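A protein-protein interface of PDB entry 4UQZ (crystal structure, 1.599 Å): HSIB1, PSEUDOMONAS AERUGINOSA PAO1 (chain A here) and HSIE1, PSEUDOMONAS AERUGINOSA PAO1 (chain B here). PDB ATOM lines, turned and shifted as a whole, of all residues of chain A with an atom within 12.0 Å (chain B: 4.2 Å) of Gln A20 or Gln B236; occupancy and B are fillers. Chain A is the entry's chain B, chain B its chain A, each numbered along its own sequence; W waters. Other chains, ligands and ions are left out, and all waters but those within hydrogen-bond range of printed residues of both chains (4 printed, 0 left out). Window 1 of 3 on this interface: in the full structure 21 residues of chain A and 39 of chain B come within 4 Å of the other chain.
OE1 of Glu A22 lies within salt-bridge range of NE of Arg B223, at 3.8 Å. The backbone carbonyl oxygen (O) of Thr B225 sits at hydrogen-bond distance from the backbone NH (N) of Arg A18 (2.8 Å). The side-chain amide nitrogen (NE2) of Gln A20 lies within hydrogen-bond range of the side-chain hydroxyl (OG1) of Thr B225 (2.9 Å). The side-chain hydroxyl (OH) of Tyr A23 sits at hydrogen-bond distance from the backbone carbonyl oxygen (O) of Phe B249, 3.3 Å away.
The backbone carbonyl oxygen (O) of Gly B222 is in hydrogen-bond range of the side-chain amide nitrogen (NE2) of Gln B236 (2.9 Å). O of Lys B224 sits at hydrogen-bond distance from N of Gln B236. The side-chain hydroxyl of Thr B225 lies within hydrogen-bond range of the backbone carbonyl oxygen of Gln B236 (2.6 Å). The backbone NH (N) of Leu B248 sits at hydrogen-bond distance from the side-chain amide oxygen (OE1) of Gln B236. The backbone NH (N) of Phe B249 sits at hydrogen-bond distance from the side-chain amide oxygen (OE1) of Gln B236. The backbone carbonyl oxygen (O) of Ala A16 is in hydrogen-bond range of the guanidinium group (NH1) of Arg A18.
Among the printed residues, pairs that only touch across the chains: Arg A18 with Lys B224, Pro A17 with Thr B225, Gln A20 with Ala B247, Gln A20 with Arg B223, Gln A20 with Gln B236, Gln A20 with Lys B224 and Arg A18 with Leu B238.
Of the printed residues of chain B, Arg A18 touches Lys B224, Thr B225 and Leu B238. Of chain B, only Arg B223, Lys B224, Thr B225, Gln B236 and Ala B247 come within 4 Å of Gln A20. Printed residues of chain B within 4 Å of Glu A22: Arg B223 (3.5 Å). Printed residues of chain B within 4 Å of Tyr A23: Phe B249. No residue of chain A comes within 4 Å of Ala B206. No residue of chain A comes within 4 Å of Tyr B208. No residue of chain A comes within 4 Å of Gly B222. Of the printed residues of chain A, Lys B224 touches Arg A18 and Gln A20. No residue of chain A comes within 4 Å of Gly B235. Printed residues of chain A within 4 Å of Gln B236: Gln A20. No residue of chain A comes within 4 Å of Arg B237. Phe B249 touches just one residue of chain A: Tyr A23 (3.3 Å). The nearest residue of chain A that does not touch Gln B236 is Ile A21 (4.8 Å).
Of the 13 printed residues of chain B, 7 touch a printed residue of chain A. Along chain B the printed residues that touch a printed residue of chain A span positions 223 to 249. Of the 13 printed residues of chain A, 5 touch a printed residue of chain B. Among the printed residues, Asp or Glu carboxylates within 4 Å of a Lys or Arg side-chain nitrogen of the other chain: Glu A22 with Arg B223.
Water W4 bridges O of Arg B223 (2.7 Å) and N of Gln A20 (3.1 Å). Water W2 lies within hydrogen-bond range of the backbone carbonyl oxygen (O) of Gly B222 (2.7 Å) and the backbone carbonyl oxygen (O) of Ile A21 (2.7 Å). Water W3 lies within hydrogen-bond range of the backbone carbonyl oxygen (O) of Ile A21 (2.8 Å) and the side-chain amide nitrogen (NE2) of Gln B236 (3.0 Å). Water W1 lies within hydrogen-bond range of the backbone carbonyl oxygen (O) of Tyr A23 and the guanidinium group (NH2) of Arg B223.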
ATOM      1  N   ALA A  12       3.993 -27.443  15.369  1.00  0.00           N
ATOM      2  CA  ALA A  12       2.946 -26.438  15.275  1.00  0.00           C
ATOM      3  C   ALA A  12       1.601 -27.110  15.058  1.00  0.00           C
ATOM      4  O   ALA A  12       1.426 -27.896  14.129  1.00  0.00           O
ATOM      5  CB  ALA A  12       3.220 -25.452  14.141  1.00  0.00           C
ATOM      6  N   ASN A  14      -1.218 -25.653  14.262  1.00  0.00           N
ATOM      7  CA  ASN A  14      -2.024 -24.933  13.288  1.00  0.00           C
ATOM      8  C   ASN A  14      -1.147 -24.484  12.113  1.00  0.00           C
ATOM      9  O   ASN A  14      -0.110 -23.906  12.347  1.00  0.00           O
ATOM     10  CB  ASN A  14      -2.697 -23.734  13.995  1.00  0.00           C
ATOM     11  CG  ASN A  14      -3.155 -22.648  13.045  1.00  0.00           C
ATOM     12  OD1 ASN A  14      -3.512 -22.911  11.903  1.00  0.00           O
ATOM     13  ND2 ASN A  14      -3.185 -21.408  13.538  1.00  0.00           N
ATOM     14  N   ARG A  15      -1.544 -24.781  10.874  1.00  0.00           N
ATOM     15  CA  ARG A  15      -0.808 -24.267   9.711  1.00  0.00           C
ATOM     16  C   ARG A  15      -1.653 -23.327   8.854  1.00  0.00           C
ATOM     17  O   ARG A  15      -1.427 -23.197   7.645  1.00  0.00           O
ATOM     18  CB  ARG A  15      -0.267 -25.421   8.863  1.00  0.00           C
ATOM     19  CG  ARG A  15       0.785 -26.246   9.584  1.00  0.00           C
ATOM     20  CD  ARG A  15       1.240 -27.392   8.703  1.00  0.00           C
ATOM     21  NE  ARG A  15       2.665 -27.675   8.837  1.00  0.00           N
ATOM     22  CZ  ARG A  15       3.399 -28.197   7.858  1.00  0.00           C
ATOM     23  NH1 ARG A  15       2.828 -28.481   6.693  1.00  0.00           N
ATOM     24  NH2 ARG A  15       4.693 -28.443   8.037  1.00  0.00           N
ATOM     25  N   ALA A  16      -2.596 -22.648   9.492  1.00  0.00           N
ATOM     26  CA  ALA A  16      -3.346 -21.587   8.837  1.00  0.00           C
ATOM     27  C   ALA A  16      -2.442 -20.376   8.683  1.00  0.00           C
ATOM     28  O   ALA A  16      -1.493 -20.186   9.466  1.00  0.00           O
ATOM     29  CB  ALA A  16      -4.560 -21.223   9.629  1.00  0.00           C
ATOM     30  N   PRO A  17      -2.733 -19.530   7.688  1.00  0.00           N
ATOM     31  CA  PRO A  17      -1.918 -18.313   7.588  1.00  0.00           C
ATOM     32  C   PRO A  17      -1.951 -17.447   8.843  1.00  0.00           C
ATOM     33  O   PRO A  17      -3.003 -17.333   9.503  1.00  0.00           O
ATOM     34  CB  PRO A  17      -2.560 -17.553   6.408  1.00  0.00           C
ATOM     35  CG  PRO A  17      -3.265 -18.601   5.596  1.00  0.00           C
ATOM     36  CD  PRO A  17      -3.734 -19.638   6.608  1.00  0.00           C
ATOM     37  N   ARG A  18      -0.840 -16.794   9.143  1.00  0.00           N
ATOM     38  CA  ARG A  18      -0.722 -15.912  10.291  1.00  0.00           C
ATOM     39  C   ARG A  18      -0.607 -14.476   9.845  1.00  0.00           C
ATOM     40  O   ARG A  18       0.271 -14.133   9.024  1.00  0.00           O
ATOM     41  CB  ARG A  18       0.513 -16.259  11.154  1.00  0.00           C
ATOM     42  CG  ARG A  18       0.686 -17.751  11.473  1.00  0.00           C
ATOM     43  CD  ARG A  18      -0.434 -18.319  12.195  1.00  0.00           C
ATOM     44  NE  ARG A  18       0.037 -19.330  13.148  1.00  0.00           N
ATOM     45  CZ  ARG A  18       0.127 -20.635  12.886  1.00  0.00           C
ATOM     46  NH1 ARG A  18      -0.202 -21.109  11.690  1.00  0.00           N
ATOM     47  NH2 ARG A  18       0.534 -21.478  13.834  1.00  0.00           N
ATOM     48  N   VAL A  19      -1.505 -13.629  10.337  1.00  0.00           N
ATOM     49  CA  VAL A  19      -1.381 -12.198  10.126  1.00  0.00           C
ATOM     50  C   VAL A  19      -0.348 -11.716  11.144  1.00  0.00           C
ATOM     51  O   VAL A  19      -0.214 -12.293  12.217  1.00  0.00           O
ATOM     52  CB  VAL A  19      -2.743 -11.500  10.298  1.00  0.00           C
ATOM     53  CG1 VAL A  19      -3.730 -12.101   9.305  1.00  0.00           C
ATOM     54  CG2 VAL A  19      -3.244 -11.652  11.710  1.00  0.00           C
ATOM     55  N   GLN A  20       0.466 -10.735  10.777  1.00  0.00           N
ATOM     56  CA  GLN A  20       1.555 -10.300  11.644  1.00  0.00           C
ATOM     57  C   GLN A  20       1.485  -8.814  11.878  1.00  0.00           C
ATOM     58  O   GLN A  20       0.833  -8.077  11.099  1.00  0.00           O
ATOM     59  CB  GLN A  20       2.931 -10.623  11.032  1.00  0.00           C
ATOM     60  CG  GLN A  20       3.164 -12.088  10.655  1.00  0.00           C
ATOM     61  CD  GLN A  20       3.363 -13.000  11.863  1.00  0.00           C
ATOM     62  OE1 GLN A  20       3.153 -12.598  13.006  1.00  0.00           O
ATOM     63  NE2 GLN A  20       3.825 -14.232  11.607  1.00  0.00           N
ATOM     64  N   ILE A  21       2.136  -8.390  12.951  1.00  0.00           N
ATOM     65  CA  ILE A  21       2.461  -6.990  13.192  1.00  0.00           C
ATOM     66  C   ILE A  21       3.404  -6.525  12.098  1.00  0.00           C
ATOM     67  O   ILE A  21       4.383  -7.205  11.794  1.00  0.00           O
ATOM     68  CB  ILE A  21       3.144  -6.800  14.545  1.00  0.00           C
ATOM     69  CG1 ILE A  21       2.231  -7.277  15.694  1.00  0.00           C
ATOM     70  CG2 ILE A  21       3.628  -5.378  14.748  1.00  0.00           C
ATOM     71  CD1 ILE A  21       2.942  -7.287  17.022  1.00  0.00           C
ATOM     72  N   GLU A  22       3.114  -5.368  11.509  1.00  0.00           N
ATOM     73  CA  GLU A  22       4.022  -4.804  10.507  1.00  0.00           C
ATOM     74  C   GLU A  22       4.860  -3.711  11.149  1.00  0.00           C
ATOM     75  O   GLU A  22       4.394  -2.981  12.021  1.00  0.00           O
ATOM     76  CB  GLU A  22       3.206  -4.310   9.303  1.00  0.00           C
ATOM     77  CG  GLU A  22       2.362  -5.472   8.722  1.00  0.00           C
ATOM     78  CD  GLU A  22       1.587  -5.115   7.458  1.00  0.00           C
ATOM     79  OE1 GLU A  22       1.861  -4.038   6.881  1.00  0.00           O
ATOM     80  OE2 GLU A  22       0.726  -5.932   7.044  1.00  0.00           O
ATOM     81  N   TYR A  23       6.126  -3.632  10.753  1.00  0.00           N
ATOM     82  CA  TYR A  23       7.076  -2.683  11.332  1.00  0.00           C
ATOM     83  C   TYR A  23       7.463  -1.641  10.296  1.00  0.00           C
ATOM     84  O   TYR A  23       7.738  -1.981   9.149  1.00  0.00           O
ATOM     85  CB  TYR A  23       8.336  -3.398  11.854  1.00  0.00           C
ATOM     86  CG  TYR A  23       8.024  -4.282  13.046  1.00  0.00           C
ATOM     87  CD1 TYR A  23       8.026  -3.757  14.330  1.00  0.00           C
ATOM     88  CD2 TYR A  23       7.684  -5.633  12.885  1.00  0.00           C
ATOM     89  CE1 TYR A  23       7.698  -4.547  15.446  1.00  0.00           C
ATOM     90  CE2 TYR A  23       7.385  -6.431  13.989  1.00  0.00           C
ATOM     91  CZ  TYR A  23       7.421  -5.889  15.273  1.00  0.00           C
ATOM     92  OH  TYR A  23       7.082  -6.653  16.389  1.00  0.00           O
ATOM     93  N   ASP A  24       7.457  -0.381  10.709  1.00  0.00           N
ATOM     94  CA  ASP A  24       7.955   0.694   9.853  1.00  0.00           C
ATOM     95  C   ASP A  24       9.472   0.686   9.975  1.00  0.00           C
ATOM     96  O   ASP A  24      10.015   0.742  11.074  1.00  0.00           O
ATOM     97  CB  ASP A  24       7.352   2.035  10.269  1.00  0.00           C
ATOM     98  CG  ASP A  24       7.868   3.199   9.430  1.00  0.00           C
ATOM     99  OD1 ASP A  24       7.807   3.129   8.178  1.00  0.00           O
ATOM    100  OD2 ASP A  24       8.350   4.179  10.035  1.00  0.00           O
ATOM    101  N   VAL A  25      10.179   0.528   8.865  1.00  0.00           N
ATOM    102  CA  VAL A  25      11.609   0.373   8.980  1.00  0.00           C
ATOM    103  C   VAL A  25      12.296   1.505   8.254  1.00  0.00           C
ATOM    104  O   VAL A  25      11.701   2.142   7.370  1.00  0.00           O
ATOM    105  CB  VAL A  25      12.093  -0.979   8.409  1.00  0.00           C
ATOM    106  CG1 VAL A  25      11.560  -2.109   9.258  1.00  0.00           C
ATOM    107  CG2 VAL A  25      11.619  -1.144   6.990  1.00  0.00           C
ATOM    108  N   ALA B 206      15.580 -14.386   8.593  1.00  0.00           N
ATOM    109  CA  ALA B 206      14.322 -14.058   9.253  1.00  0.00           C
ATOM    110  C   ALA B 206      13.112 -14.560   8.486  1.00  0.00           C
ATOM    111  O   ALA B 206      11.978 -14.506   8.998  1.00  0.00           O
ATOM    112  CB  ALA B 206      14.226 -12.553   9.475  1.00  0.00           C
ATOM    113  N   TYR B 208      11.532 -17.761   5.820  1.00  0.00           N
ATOM    114  CA  TYR B 208      11.789 -19.114   5.315  1.00  0.00           C
ATOM    115  C   TYR B 208      12.467 -19.065   3.953  1.00  0.00           C
ATOM    116  O   TYR B 208      12.262 -18.146   3.156  1.00  0.00           O
ATOM    117  CB  TYR B 208      10.489 -19.933   5.273  1.00  0.00           C
ATOM    118  CG  TYR B 208      10.040 -20.122   6.710  1.00  0.00           C
ATOM    119  CD1 TYR B 208      10.773 -20.922   7.574  1.00  0.00           C
ATOM    120  CD2 TYR B 208       8.932 -19.455   7.228  1.00  0.00           C
ATOM    121  CE1 TYR B 208      10.419 -21.086   8.909  1.00  0.00           C
ATOM    122  CE2 TYR B 208       8.550 -19.615   8.565  1.00  0.00           C
ATOM    123  CZ  TYR B 208       9.297 -20.455   9.409  1.00  0.00           C
ATOM    124  OH  TYR B 208       8.968 -20.594  10.728  1.00  0.00           O
ATOM    125  N   GLY B 222       7.882 -10.150   5.239  1.00  0.00           N
ATOM    126  CA  GLY B 222       7.669 -10.706   6.595  1.00  0.00           C
ATOM    127  C   GLY B 222       6.368 -10.267   7.276  1.00  0.00           C
ATOM    128  O   GLY B 222       6.254 -10.305   8.504  1.00  0.00           O
ATOM    129  N   ARG B 223       5.385  -9.855   6.471  1.00  0.00           N
ATOM    130  CA  ARG B 223       4.106  -9.340   6.956  1.00  0.00           C
ATOM    131  C   ARG B 223       3.074 -10.447   7.133  1.00  0.00           C
ATOM    132  O   ARG B 223       1.961 -10.218   7.624  1.00  0.00           O
ATOM    133  CB  ARG B 223       3.605  -8.275   5.989  1.00  0.00           C
ATOM    134  CG  ARG B 223       4.534  -7.084   5.938  1.00  0.00           C
ATOM    135  CD  ARG B 223       4.044  -6.029   4.980  1.00  0.00           C
ATOM    136  NE  ARG B 223       4.966  -4.915   4.943  1.00  0.00           N
ATOM    137  CZ  ARG B 223       4.815  -3.861   4.137  1.00  0.00           C
ATOM    138  NH1 ARG B 223       3.784  -3.802   3.312  1.00  0.00           N
ATOM    139  NH2 ARG B 223       5.689  -2.876   4.156  1.00  0.00           N
ATOM    140  N   LYS B 224       3.448 -11.665   6.745  1.00  0.00           N
ATOM    141  CA  LYS B 224       2.613 -12.832   7.029  1.00  0.00           C
ATOM    142  C   LYS B 224       3.486 -14.065   7.104  1.00  0.00           C
ATOM    143  O   LYS B 224       4.648 -14.027   6.687  1.00  0.00           O
ATOM    144  CB  LYS B 224       1.548 -13.013   5.958  1.00  0.00           C
ATOM    145  CG  LYS B 224       2.107 -13.301   4.591  1.00  0.00           C
ATOM    146  CD  LYS B 224       0.921 -13.704   3.716  1.00  0.00           C
ATOM    147  CE  LYS B 224       1.263 -13.742   2.293  1.00  0.00           C
ATOM    148  NZ  LYS B 224       0.053 -14.105   1.467  1.00  0.00           N
ATOM    149  N   THR B 225       2.935 -15.150   7.647  1.00  0.00           N
ATOM    150  CA  THR B 225       3.540 -16.468   7.557  1.00  0.00           C
ATOM    151  C   THR B 225       2.469 -17.402   7.037  1.00  0.00           C
ATOM    152  O   THR B 225       1.323 -17.363   7.517  1.00  0.00           O
ATOM    153  CB  THR B 225       4.012 -16.939   8.917  1.00  0.00           C
ATOM    154  OG1 THR B 225       4.869 -15.963   9.508  1.00  0.00           O
ATOM    155  CG2 THR B 225       4.730 -18.314   8.864  1.00  0.00           C
ATOM    156  N   GLY B 235       7.367 -16.656   4.285  1.00  0.00           N
ATOM    157  CA  GLY B 235       7.131 -15.498   5.108  1.00  0.00           C
ATOM    158  C   GLY B 235       7.977 -15.470   6.360  1.00  0.00           C
ATOM    159  O   GLY B 235       9.053 -16.123   6.476  1.00  0.00           O
ATOM    160  N   GLN B 236       7.488 -14.740   7.345  1.00  0.00           N
ATOM    161  CA  GLN B 236       8.232 -14.521   8.574  1.00  0.00           C
ATOM    162  C   GLN B 236       8.394 -15.775   9.424  1.00  0.00           C
ATOM    163  O   GLN B 236       7.451 -16.519   9.641  1.00  0.00           O
ATOM    164  CB  GLN B 236       7.561 -13.432   9.411  1.00  0.00           C
ATOM    165  CG  GLN B 236       8.416 -13.007  10.571  1.00  0.00           C
ATOM    166  CD  GLN B 236       7.725 -12.131  11.574  1.00  0.00           C
ATOM    167  OE1 GLN B 236       8.147 -12.068  12.732  1.00  0.00           O
ATOM    168  NE2 GLN B 236       6.687 -11.391  11.144  1.00  0.00           N
ATOM    169  N   ARG B 237       9.624 -15.982   9.898  1.00  0.00           N
ATOM    170  CA  ARG B 237       9.895 -17.067  10.859  1.00  0.00           C
ATOM    171  C   ARG B 237       8.963 -17.016  12.082  1.00  0.00           C
ATOM    172  O   ARG B 237       8.760 -15.970  12.735  1.00  0.00           O
ATOM    173  CB  ARG B 237      11.361 -17.020  11.298  1.00  0.00           C
ATOM    174  CG  ARG B 237      11.745 -18.257  12.077  1.00  0.00           C
ATOM    175  CD  ARG B 237      13.220 -18.298  12.318  1.00  0.00           C
ATOM    176  NE  ARG B 237      13.988 -18.243  11.085  1.00  0.00           N
ATOM    177  CZ  ARG B 237      14.136 -19.243  10.206  1.00  0.00           C
ATOM    178  NH1 ARG B 237      13.528 -20.442  10.339  1.00  0.00           N
ATOM    179  NH2 ARG B 237      14.915 -19.033   9.140  1.00  0.00           N
ATOM    180  N   LEU B 238       8.461 -18.205  12.411  1.00  0.00           N
ATOM    181  CA  LEU B 238       7.528 -18.404  13.508  1.00  0.00           C
ATOM    182  C   LEU B 238       8.076 -19.458  14.454  1.00  0.00           C
ATOM    183  O   LEU B 238       8.504 -20.520  14.004  1.00  0.00           O
ATOM    184  CB  LEU B 238       6.154 -18.844  12.978  1.00  0.00           C
ATOM    185  CG  LEU B 238       5.035 -19.052  13.989  1.00  0.00           C
ATOM    186  CD1 LEU B 238       4.671 -17.751  14.675  1.00  0.00           C
ATOM    187  CD2 LEU B 238       3.850 -19.628  13.220  1.00  0.00           C
ATOM    188  N   ALA B 247       6.241 -14.900  16.605  1.00  0.00           N
ATOM    189  CA  ALA B 247       6.970 -14.604  15.392  1.00  0.00           C
ATOM    190  C   ALA B 247       8.314 -13.958  15.725  1.00  0.00           C
ATOM    191  O   ALA B 247       8.427 -13.245  16.728  1.00  0.00           O
ATOM    192  CB  ALA B 247       6.102 -13.679  14.492  1.00  0.00           C
ATOM    193  N   LEU B 248       9.328 -14.243  14.902  1.00  0.00           N
ATOM    194  CA  LEU B 248      10.680 -13.780  15.166  1.00  0.00           C
ATOM    195  C   LEU B 248      10.769 -12.258  15.354  1.00  0.00           C
ATOM    196  O   LEU B 248      11.440 -11.781  16.287  1.00  0.00           O
ATOM    197  CB  LEU B 248      11.618 -14.221  14.042  1.00  0.00           C
ATOM    198  CG  LEU B 248      13.016 -13.606  14.091  1.00  0.00           C
ATOM    199  CD1 LEU B 248      13.766 -14.108  15.308  1.00  0.00           C
ATOM    200  CD2 LEU B 248      13.735 -13.999  12.790  1.00  0.00           C
ATOM    201  N   PHE B 249      10.071 -11.481  14.508  1.00  0.00           N
ATOM    202  CA  PHE B 249      10.154 -10.004  14.641  1.00  0.00           C
ATOM    203  C   PHE B 249       9.605  -9.497  15.985  1.00  0.00           C
ATOM    204  O   PHE B 249       9.853  -8.370  16.372  1.00  0.00           O
ATOM    205  CB  PHE B 249       9.383  -9.272  13.538  1.00  0.00           C
ATOM    206  CG  PHE B 249       9.936  -9.467  12.164  1.00  0.00           C
ATOM    207  CD1 PHE B 249      11.223  -9.946  11.965  1.00  0.00           C
ATOM    208  CD2 PHE B 249       9.166  -9.136  11.053  1.00  0.00           C
ATOM    209  CE1 PHE B 249      11.724 -10.083  10.665  1.00  0.00           C
ATOM    210  CE2 PHE B 249       9.645  -9.297   9.777  1.00  0.00           C
ATOM    211  CZ  PHE B 249      10.916  -9.783   9.582  1.00  0.00           C
HETATM  212  O   HOH W   1       8.103  -2.913   6.456  1.00  0.00           O
HETATM  213  O   HOH W   2       5.890  -7.878   9.639  1.00  0.00           O
HETATM  214  O   HOH W   3       5.708  -9.366  13.070  1.00  0.00           O
HETATM  215  O   HOH W   4      -0.624  -9.791   8.049  1.00  0.00           O
